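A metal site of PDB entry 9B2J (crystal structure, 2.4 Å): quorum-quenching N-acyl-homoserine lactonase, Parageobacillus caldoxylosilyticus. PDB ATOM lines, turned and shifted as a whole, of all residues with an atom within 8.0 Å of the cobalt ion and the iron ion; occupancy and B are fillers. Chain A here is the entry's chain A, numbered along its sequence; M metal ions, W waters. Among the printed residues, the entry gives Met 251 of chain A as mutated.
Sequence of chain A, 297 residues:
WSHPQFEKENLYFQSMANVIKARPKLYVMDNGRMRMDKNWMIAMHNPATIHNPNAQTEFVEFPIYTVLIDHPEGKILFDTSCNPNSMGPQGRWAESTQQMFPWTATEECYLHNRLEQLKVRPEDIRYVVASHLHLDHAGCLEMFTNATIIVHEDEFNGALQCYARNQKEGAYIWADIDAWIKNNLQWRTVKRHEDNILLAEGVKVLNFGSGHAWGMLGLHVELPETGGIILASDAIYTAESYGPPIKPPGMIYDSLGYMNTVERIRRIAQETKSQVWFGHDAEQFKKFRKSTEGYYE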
ATOM      1  N   MET A  34       6.883  26.609  19.058  1.00  0.00           N
ATOM      2  CA  MET A  34       7.108  25.206  19.394  1.00  0.00           C
ATOM      3  C   MET A  34       6.016  24.361  18.724  1.00  0.00           C
ATOM      4  O   MET A  34       4.912  24.862  18.518  1.00  0.00           O
ATOM      5  CB  MET A  34       7.053  24.987  20.910  1.00  0.00           C
ATOM      6  CG  MET A  34       7.206  23.539  21.368  1.00  0.00           C
ATOM      7  SD  MET A  34       7.345  23.365  23.162  1.00  0.00           S
ATOM      8  CE  MET A  34       8.945  24.124  23.453  1.00  0.00           C
ATOM      9  N   MET A  36       4.130  20.226  18.714  1.00  0.00           N
ATOM     10  CA  MET A  36       3.962  18.985  19.461  1.00  0.00           C
ATOM     11  C   MET A  36       2.636  18.290  19.098  1.00  0.00           C
ATOM     12  O   MET A  36       1.768  18.907  18.490  1.00  0.00           O
ATOM     13  CB  MET A  36       3.977  19.238  20.971  1.00  0.00           C
ATOM     14  CG  MET A  36       2.704  19.850  21.516  1.00  0.00           C
ATOM     15  SD  MET A  36       2.785  20.187  23.284  1.00  0.00           S
ATOM     16  CE  MET A  36       1.124  20.810  23.597  1.00  0.00           C
ATOM     17  N   PHE A  62       2.398  26.374  18.051  1.00  0.00           N
ATOM     18  CA  PHE A  62       1.878  27.343  19.011  1.00  0.00           C
ATOM     19  C   PHE A  62       3.004  28.279  19.448  1.00  0.00           C
ATOM     20  O   PHE A  62       4.172  27.918  19.391  1.00  0.00           O
ATOM     21  CB  PHE A  62       1.234  26.648  20.226  1.00  0.00           C
ATOM     22  CG  PHE A  62       2.160  25.697  20.969  1.00  0.00           C
ATOM     23  CD1 PHE A  62       2.970  26.151  22.008  1.00  0.00           C
ATOM     24  CD2 PHE A  62       2.224  24.354  20.628  1.00  0.00           C
ATOM     25  CE1 PHE A  62       3.804  25.277  22.680  1.00  0.00           C
ATOM     26  CE2 PHE A  62       3.066  23.483  21.306  1.00  0.00           C
ATOM     27  CZ  PHE A  62       3.857  23.945  22.332  1.00  0.00           C
ATOM     28  N   PRO A  63       2.685  29.522  19.890  1.00  0.00           N
ATOM     29  CA  PRO A  63       3.699  30.498  20.283  1.00  0.00           C
ATOM     30  C   PRO A  63       4.215  30.350  21.721  1.00  0.00           C
ATOM     31  O   PRO A  63       3.444  30.018  22.613  1.00  0.00           O
ATOM     32  CB  PRO A  63       2.951  31.833  20.102  1.00  0.00           C
ATOM     33  CG  PRO A  63       1.507  31.497  20.438  1.00  0.00           C
ATOM     34  CD  PRO A  63       1.307  30.041  20.019  1.00  0.00           C
ATOM     35  N   ILE A  64       5.521  30.602  21.902  1.00  0.00           N
ATOM     36  CA  ILE A  64       6.138  30.804  23.205  1.00  0.00           C
ATOM     37  C   ILE A  64       6.315  32.312  23.417  1.00  0.00           C
ATOM     38  O   ILE A  64       6.907  32.979  22.556  1.00  0.00           O
ATOM     39  CB  ILE A  64       7.492  30.067  23.286  1.00  0.00           C
ATOM     40  CG1 ILE A  64       7.407  28.617  22.812  1.00  0.00           C
ATOM     41  CG2 ILE A  64       8.097  30.171  24.691  1.00  0.00           C
ATOM     42  CD1 ILE A  64       6.307  27.805  23.490  1.00  0.00           C
ATOM     43  N   ASP A  79       7.373  34.799  33.187  1.00  0.00           N
ATOM     44  CA  ASP A  79       7.921  33.705  32.373  1.00  0.00           C
ATOM     45  C   ASP A  79       9.215  34.138  31.700  1.00  0.00           C
ATOM     46  O   ASP A  79       9.529  35.330  31.679  1.00  0.00           O
ATOM     47  CB  ASP A  79       6.875  33.138  31.414  1.00  0.00           C
ATOM     48  CG  ASP A  79       5.895  32.142  32.033  1.00  0.00           C
ATOM     49  OD1 ASP A  79       6.146  31.702  33.180  1.00  0.00           O
ATOM     50  OD2 ASP A  79       4.888  31.826  31.361  1.00  0.00           O
ATOM     51  N   SER A 131       5.621  30.930  36.133  1.00  0.00           N
ATOM     52  CA  SER A 131       4.298  30.306  36.156  1.00  0.00           C
ATOM     53  C   SER A 131       4.429  28.846  36.562  1.00  0.00           C
ATOM     54  O   SER A 131       3.654  28.357  37.395  1.00  0.00           O
ATOM     55  CB  SER A 131       3.580  30.466  34.835  1.00  0.00           C
ATOM     56  OG  SER A 131       4.227  29.745  33.790  1.00  0.00           O
ATOM     57  N   HIS A 132       5.402  28.151  35.959  1.00  0.00           N
ATOM     58  CA  HIS A 132       5.856  26.813  36.355  1.00  0.00           C
ATOM     59  C   HIS A 132       7.258  26.618  35.784  1.00  0.00           C
ATOM     60  O   HIS A 132       7.808  27.556  35.186  1.00  0.00           O
ATOM     61  CB  HIS A 132       4.832  25.735  35.987  1.00  0.00           C
ATOM     62  CG  HIS A 132       4.498  25.641  34.541  1.00  0.00           C
ATOM     63  ND1 HIS A 132       4.185  26.747  33.778  1.00  0.00           N
ATOM     64  CD2 HIS A 132       4.394  24.584  33.725  1.00  0.00           C
ATOM     65  CE1 HIS A 132       3.919  26.368  32.537  1.00  0.00           C
ATOM     66  NE2 HIS A 132       4.038  25.050  32.479  1.00  0.00           N
ATOM     67  N   LEU A 133       7.863  25.424  35.953  1.00  0.00           N
ATOM     68  CA  LEU A 133       9.282  25.244  35.655  1.00  0.00           C
ATOM     69  C   LEU A 133       9.492  24.306  34.468  1.00  0.00           C
ATOM     70  O   LEU A 133      10.539  23.665  34.359  1.00  0.00           O
ATOM     71  CB  LEU A 133      10.003  24.744  36.908  1.00  0.00           C
ATOM     72  CG  LEU A 133      10.009  25.720  38.095  1.00  0.00           C
ATOM     73  CD1 LEU A 133      10.769  25.161  39.286  1.00  0.00           C
ATOM     74  CD2 LEU A 133      10.592  27.068  37.680  1.00  0.00           C
ATOM     75  N   HIS A 134       8.518  24.277  33.540  1.00  0.00           N
ATOM     76  CA  HIS A 134       8.630  23.568  32.272  1.00  0.00           C
ATOM     77  C   HIS A 134       9.660  24.264  31.375  1.00  0.00           C
ATOM     78  O   HIS A 134       9.963  25.441  31.572  1.00  0.00           O
ATOM     79  CB  HIS A 134       7.264  23.484  31.576  1.00  0.00           C
ATOM     80  CG  HIS A 134       6.373  22.390  32.083  1.00  0.00           C
ATOM     81  ND1 HIS A 134       5.044  22.308  31.744  1.00  0.00           N
ATOM     82  CD2 HIS A 134       6.632  21.331  32.861  1.00  0.00           C
ATOM     83  CE1 HIS A 134       4.523  21.233  32.314  1.00  0.00           C
ATOM     84  NE2 HIS A 134       5.470  20.625  33.004  1.00  0.00           N
ATOM     85  N   LEU A 135      10.160  23.526  30.364  1.00  0.00           N
ATOM     86  CA  LEU A 135      11.293  23.925  29.523  1.00  0.00           C
ATOM     87  C   LEU A 135      11.001  25.202  28.737  1.00  0.00           C
ATOM     88  O   LEU A 135      11.938  25.925  28.382  1.00  0.00           O
ATOM     89  CB  LEU A 135      11.658  22.760  28.587  1.00  0.00           C
ATOM     90  CG  LEU A 135      10.642  22.397  27.507  1.00  0.00           C
ATOM     91  CD1 LEU A 135      11.152  21.263  26.639  1.00  0.00           C
ATOM     92  CD2 LEU A 135       9.289  22.027  28.106  1.00  0.00           C
ATOM     93  N   ASP A 136       9.720  25.511  28.478  1.00  0.00           N
ATOM     94  CA  ASP A 136       9.326  26.619  27.614  1.00  0.00           C
ATOM     95  C   ASP A 136       8.892  27.850  28.417  1.00  0.00           C
ATOM     96  O   ASP A 136       8.402  28.813  27.827  1.00  0.00           O
ATOM     97  CB  ASP A 136       8.232  26.216  26.643  1.00  0.00           C
ATOM     98  CG  ASP A 136       6.981  25.622  27.299  1.00  0.00           C
ATOM     99  OD1 ASP A 136       7.147  24.745  28.172  1.00  0.00           O
ATOM    100  OD2 ASP A 136       5.869  26.028  26.919  1.00  0.00           O
ATOM    101  N   HIS A 137       9.082  27.827  29.748  1.00  0.00           N
ATOM    102  CA  HIS A 137       8.711  28.938  30.628  1.00  0.00           C
ATOM    103  C   HIS A 137       9.866  29.314  31.563  1.00  0.00           C
ATOM    104  O   HIS A 137       9.958  30.470  31.974  1.00  0.00           O
ATOM    105  CB  HIS A 137       7.449  28.619  31.431  1.00  0.00           C
ATOM    106  CG  HIS A 137       6.252  28.302  30.615  1.00  0.00           C
ATOM    107  ND1 HIS A 137       5.254  29.209  30.349  1.00  0.00           N
ATOM    108  CD2 HIS A 137       5.889  27.160  30.003  1.00  0.00           C
ATOM    109  CE1 HIS A 137       4.327  28.634  29.586  1.00  0.00           C
ATOM    110  NE2 HIS A 137       4.689  27.383  29.373  1.00  0.00           N
ATOM    111  N   GLU A 155       6.097  23.106  42.805  1.00  0.00           N
ATOM    112  CA  GLU A 155       6.748  23.061  41.497  1.00  0.00           C
ATOM    113  C   GLU A 155       8.266  22.997  41.680  1.00  0.00           C
ATOM    114  O   GLU A 155       8.943  22.207  41.019  1.00  0.00           O
ATOM    115  CB  GLU A 155       6.344  24.297  40.673  1.00  0.00           C
ATOM    116  CG  GLU A 155       6.849  24.278  39.235  1.00  0.00           C
ATOM    117  CD  GLU A 155       6.140  23.300  38.312  1.00  0.00           C
ATOM    118  OE1 GLU A 155       5.150  22.694  38.754  1.00  0.00           O
ATOM    119  OE2 GLU A 155       6.577  23.157  37.152  1.00  0.00           O
ATOM    120  N   ALA A 171       9.930  17.242  30.774  1.00  0.00           N
ATOM    121  CA  ALA A 171       9.696  18.673  30.597  1.00  0.00           C
ATOM    122  C   ALA A 171      10.611  19.515  31.497  1.00  0.00           C
ATOM    123  O   ALA A 171      10.630  20.737  31.373  1.00  0.00           O
ATOM    124  CB  ALA A 171       8.231  18.970  30.867  1.00  0.00           C
ATOM    125  N   TYR A 172      11.358  18.873  32.391  1.00  0.00           N
ATOM    126  CA  TYR A 172      12.215  19.556  33.358  1.00  0.00           C
ATOM    127  C   TYR A 172      13.688  19.341  32.984  1.00  0.00           C
ATOM    128  O   TYR A 172      14.227  18.263  33.206  1.00  0.00           O
ATOM    129  CB  TYR A 172      11.842  19.104  34.772  1.00  0.00           C
ATOM    130  CG  TYR A 172      10.439  19.518  35.184  1.00  0.00           C
ATOM    131  CD1 TYR A 172      10.187  20.781  35.701  1.00  0.00           C
ATOM    132  CD2 TYR A 172       9.358  18.668  35.017  1.00  0.00           C
ATOM    133  CE1 TYR A 172       8.909  21.180  36.054  1.00  0.00           C
ATOM    134  CE2 TYR A 172       8.073  19.044  35.372  1.00  0.00           C
ATOM    135  CZ  TYR A 172       7.848  20.300  35.891  1.00  0.00           C
ATOM    136  OH  TYR A 172       6.589  20.688  36.239  1.00  0.00           O
ATOM    137  N   HIS A 212      -2.158  21.427  35.729  1.00  0.00           N
ATOM    138  CA  HIS A 212      -1.247  21.171  34.608  1.00  0.00           C
ATOM    139  C   HIS A 212       0.050  20.566  35.130  1.00  0.00           C
ATOM    140  O   HIS A 212       0.524  19.562  34.605  1.00  0.00           O
ATOM    141  CB  HIS A 212      -1.018  22.463  33.802  1.00  0.00           C
ATOM    142  CG  HIS A 212       0.101  22.396  32.816  1.00  0.00           C
ATOM    143  ND1 HIS A 212       0.067  21.570  31.700  1.00  0.00           N
ATOM    144  CD2 HIS A 212       1.281  23.032  32.770  1.00  0.00           C
ATOM    145  CE1 HIS A 212       1.191  21.717  31.011  1.00  0.00           C
ATOM    146  NE2 HIS A 212       1.939  22.610  31.637  1.00  0.00           N
ATOM    147  N   ALA A 213       0.633  21.205  36.161  1.00  0.00           N
ATOM    148  CA  ALA A 213       1.873  20.787  36.796  1.00  0.00           C
ATOM    149  C   ALA A 213       1.696  20.759  38.318  1.00  0.00           C
ATOM    150  O   ALA A 213       0.578  20.850  38.811  1.00  0.00           O
ATOM    151  CB  ALA A 213       3.002  21.703  36.384  1.00  0.00           C
ATOM    152  N   MET A 216       1.067  25.868  39.867  1.00  0.00           N
ATOM    153  CA  MET A 216       0.924  26.922  38.859  1.00  0.00           C
ATOM    154  C   MET A 216       0.743  28.284  39.532  1.00  0.00           C
ATOM    155  O   MET A 216      -0.006  28.402  40.496  1.00  0.00           O
ATOM    156  CB  MET A 216      -0.301  26.666  37.963  1.00  0.00           C
ATOM    157  CG  MET A 216      -0.331  25.295  37.338  1.00  0.00           C
ATOM    158  SD  MET A 216       1.118  24.957  36.310  1.00  0.00           S
ATOM    159  CE  MET A 216       0.686  25.845  34.806  1.00  0.00           C
ATOM    160  N   SER A 233      -1.098  31.469  31.749  1.00  0.00           N
ATOM    161  CA  SER A 233      -0.061  30.543  31.313  1.00  0.00           C
ATOM    162  C   SER A 233      -0.682  29.181  30.989  1.00  0.00           C
ATOM    163  O   SER A 233      -1.743  29.124  30.372  1.00  0.00           O
ATOM    164  CB  SER A 233       1.053  30.435  32.327  1.00  0.00           C
ATOM    165  OG  SER A 233       2.141  29.671  31.811  1.00  0.00           O
ATOM    166  N   ASP A 234      -0.020  28.088  31.402  1.00  0.00           N
ATOM    167  CA  ASP A 234      -0.388  26.738  30.988  1.00  0.00           C
ATOM    168  C   ASP A 234      -1.537  26.180  31.822  1.00  0.00           C
ATOM    169  O   ASP A 234      -1.857  24.991  31.725  1.00  0.00           O
ATOM    170  CB  ASP A 234       0.813  25.811  30.982  1.00  0.00           C
ATOM    171  CG  ASP A 234       1.770  26.017  29.820  1.00  0.00           C
ATOM    172  OD1 ASP A 234       1.560  26.995  29.066  1.00  0.00           O
ATOM    173  OD2 ASP A 234       2.701  25.193  29.659  1.00  0.00           O
ATOM    174  N   ALA A 235      -2.171  27.027  32.645  1.00  0.00           N
ATOM    175  CA  ALA A 235      -3.409  26.690  33.335  1.00  0.00           C
ATOM    176  C   ALA A 235      -4.567  26.619  32.328  1.00  0.00           C
ATOM    177  O   ALA A 235      -5.528  25.884  32.543  1.00  0.00           O
ATOM    178  CB  ALA A 235      -3.691  27.693  34.430  1.00  0.00           C
ATOM    179  N   TYR A 237      -4.317  26.404  28.066  1.00  0.00           N
ATOM    180  CA  TYR A 237      -3.496  26.407  26.853  1.00  0.00           C
ATOM    181  C   TYR A 237      -4.079  27.385  25.817  1.00  0.00           C
ATOM    182  O   TYR A 237      -3.366  28.282  25.369  1.00  0.00           O
ATOM    183  CB  TYR A 237      -3.406  24.997  26.260  1.00  0.00           C
ATOM    184  CG  TYR A 237      -2.278  24.103  26.749  1.00  0.00           C
ATOM    185  CD1 TYR A 237      -1.098  24.629  27.256  1.00  0.00           C
ATOM    186  CD2 TYR A 237      -2.391  22.718  26.673  1.00  0.00           C
ATOM    187  CE1 TYR A 237      -0.064  23.805  27.681  1.00  0.00           C
ATOM    188  CE2 TYR A 237      -1.367  21.885  27.099  1.00  0.00           C
ATOM    189  CZ  TYR A 237      -0.204  22.428  27.603  1.00  0.00           C
ATOM    190  OH  TYR A 237       0.809  21.606  28.021  1.00  0.00           O
ATOM    191  N   MET A 251      -1.254  16.647  28.711  1.00  0.00           N
ATOM    192  CA  MET A 251      -0.203  16.999  29.659  1.00  0.00           C
ATOM    193  C   MET A 251      -0.838  17.578  30.916  1.00  0.00           C
ATOM    194  O   MET A 251      -1.272  18.739  30.936  1.00  0.00           O
ATOM    195  CB  MET A 251       0.810  17.986  29.071  1.00  0.00           C
ATOM    196  CG  MET A 251       2.060  18.139  29.929  1.00  0.00           C
ATOM    197  SD  MET A 251       3.369  19.113  29.151  1.00  0.00           S
ATOM    198  CE  MET A 251       3.478  18.295  27.548  1.00  0.00           C
ATOM    199  N   GLY A 279      -1.948  30.546  27.456  1.00  0.00           N
ATOM    200  CA  GLY A 279      -0.533  30.191  27.480  1.00  0.00           C
ATOM    201  C   GLY A 279       0.074  30.099  26.077  1.00  0.00           C
ATOM    202  O   GLY A 279       1.203  30.523  25.868  1.00  0.00           O
ATOM    203  N   HIS A 280      -0.705  29.542  25.135  1.00  0.00           N
ATOM    204  CA  HIS A 280      -0.194  29.090  23.845  1.00  0.00           C
ATOM    205  C   HIS A 280      -1.284  29.113  22.768  1.00  0.00           C
ATOM    206  O   HIS A 280      -1.397  28.165  22.001  1.00  0.00           O
ATOM    207  CB  HIS A 280       0.364  27.672  23.975  1.00  0.00           C
ATOM    208  CG  HIS A 280       1.539  27.551  24.894  1.00  0.00           C
ATOM    209  ND1 HIS A 280       2.709  28.243  24.694  1.00  0.00           N
ATOM    210  CD2 HIS A 280       1.746  26.791  25.990  1.00  0.00           C
ATOM    211  CE1 HIS A 280       3.583  27.928  25.645  1.00  0.00           C
ATOM    212  NE2 HIS A 280       3.008  27.050  26.443  1.00  0.00           N
HETATM  213 CO    CO M   1       3.740  23.642  30.787  1.00  0.00          CO
HETATM  214 FE    FE M   2       4.058  25.809  28.116  1.00  0.00          FE
HETATM  215  O   HOH W   1       4.958  24.119  28.828  1.00  0.00           O
HETATM  216  O   HOH W   2       3.742  23.410  26.877  1.00  0.00           O
HETATM  217  O   HOH W   3       3.387  22.449  28.853  1.00  0.00           O
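A ring nitrogen (ND1) of His 212 is in hydrogen-bond range of the backbone carbonyl oxygen (O) of Met 251 (3.2 Å).
A ring nitrogen (ND1) of His 132 sits at hydrogen-bond distance from the side-chain hydroxyl (OG) of Ser 131.
A ring nitrogen (ND1) of His 137 lies close to the side-chain hydroxyl (OG) of Ser 233 (3.5 Å).
O of Tyr 237 lies within hydrogen-bond range of N of His 280, 3.0 Å away.
The side-chain hydroxyl (OH) of Tyr 172 sits at hydrogen-bond distance from a ring nitrogen (NE2) of His 134, 3.4 Å away.
ND1 of His 280 is in hydrogen-bond range of O of Pro 63 (2.8 Å).
ND1 of His 137 sits at hydrogen-bond distance from OD2 of Asp 79, 2.8 Å away.
Within 4 Å of the cobalt ion: His 132, His 134, His 212 and Asp 234.
The nearest printed residue that does not touch the cobalt ion is His 137 (4.1 Å).
The nearest printed residue that does not touch the iron ion is His 132 (4.4 Å).
The cobalt ion is bound by ND1 of His 134 (2.1 Å), OD2 of Asp 234 (2.2 Å), NE2 of His 132 (2.2 Å), NE2 of His 212 (2.2 Å), water W3 (2.3 Å) and water W1 (2.4 Å).
The cobalt ion has six donor atoms within binding distance.
Water W1 binds the iron ion.
A ring nitrogen (NE2) of His 137 is bound to the iron ion (2.1 Å).
OD2 of Asp 234 is bound to the iron ion (2.1 Å).
The iron ion is bound by OD2 of Asp 136 (2.2 Å).
The iron ion is bound by a ring nitrogen (NE2) of His 280 (2.3 Å).
Slightly farther from the iron ion lies water W2 (2.7 Å).
Water W3 lies within hydrogen-bond range of the side-chain hydroxyl (OH) of Tyr 237 (2.8 Å) and the side-chain sulfur (SD) of Met 251 (3.3 Å).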
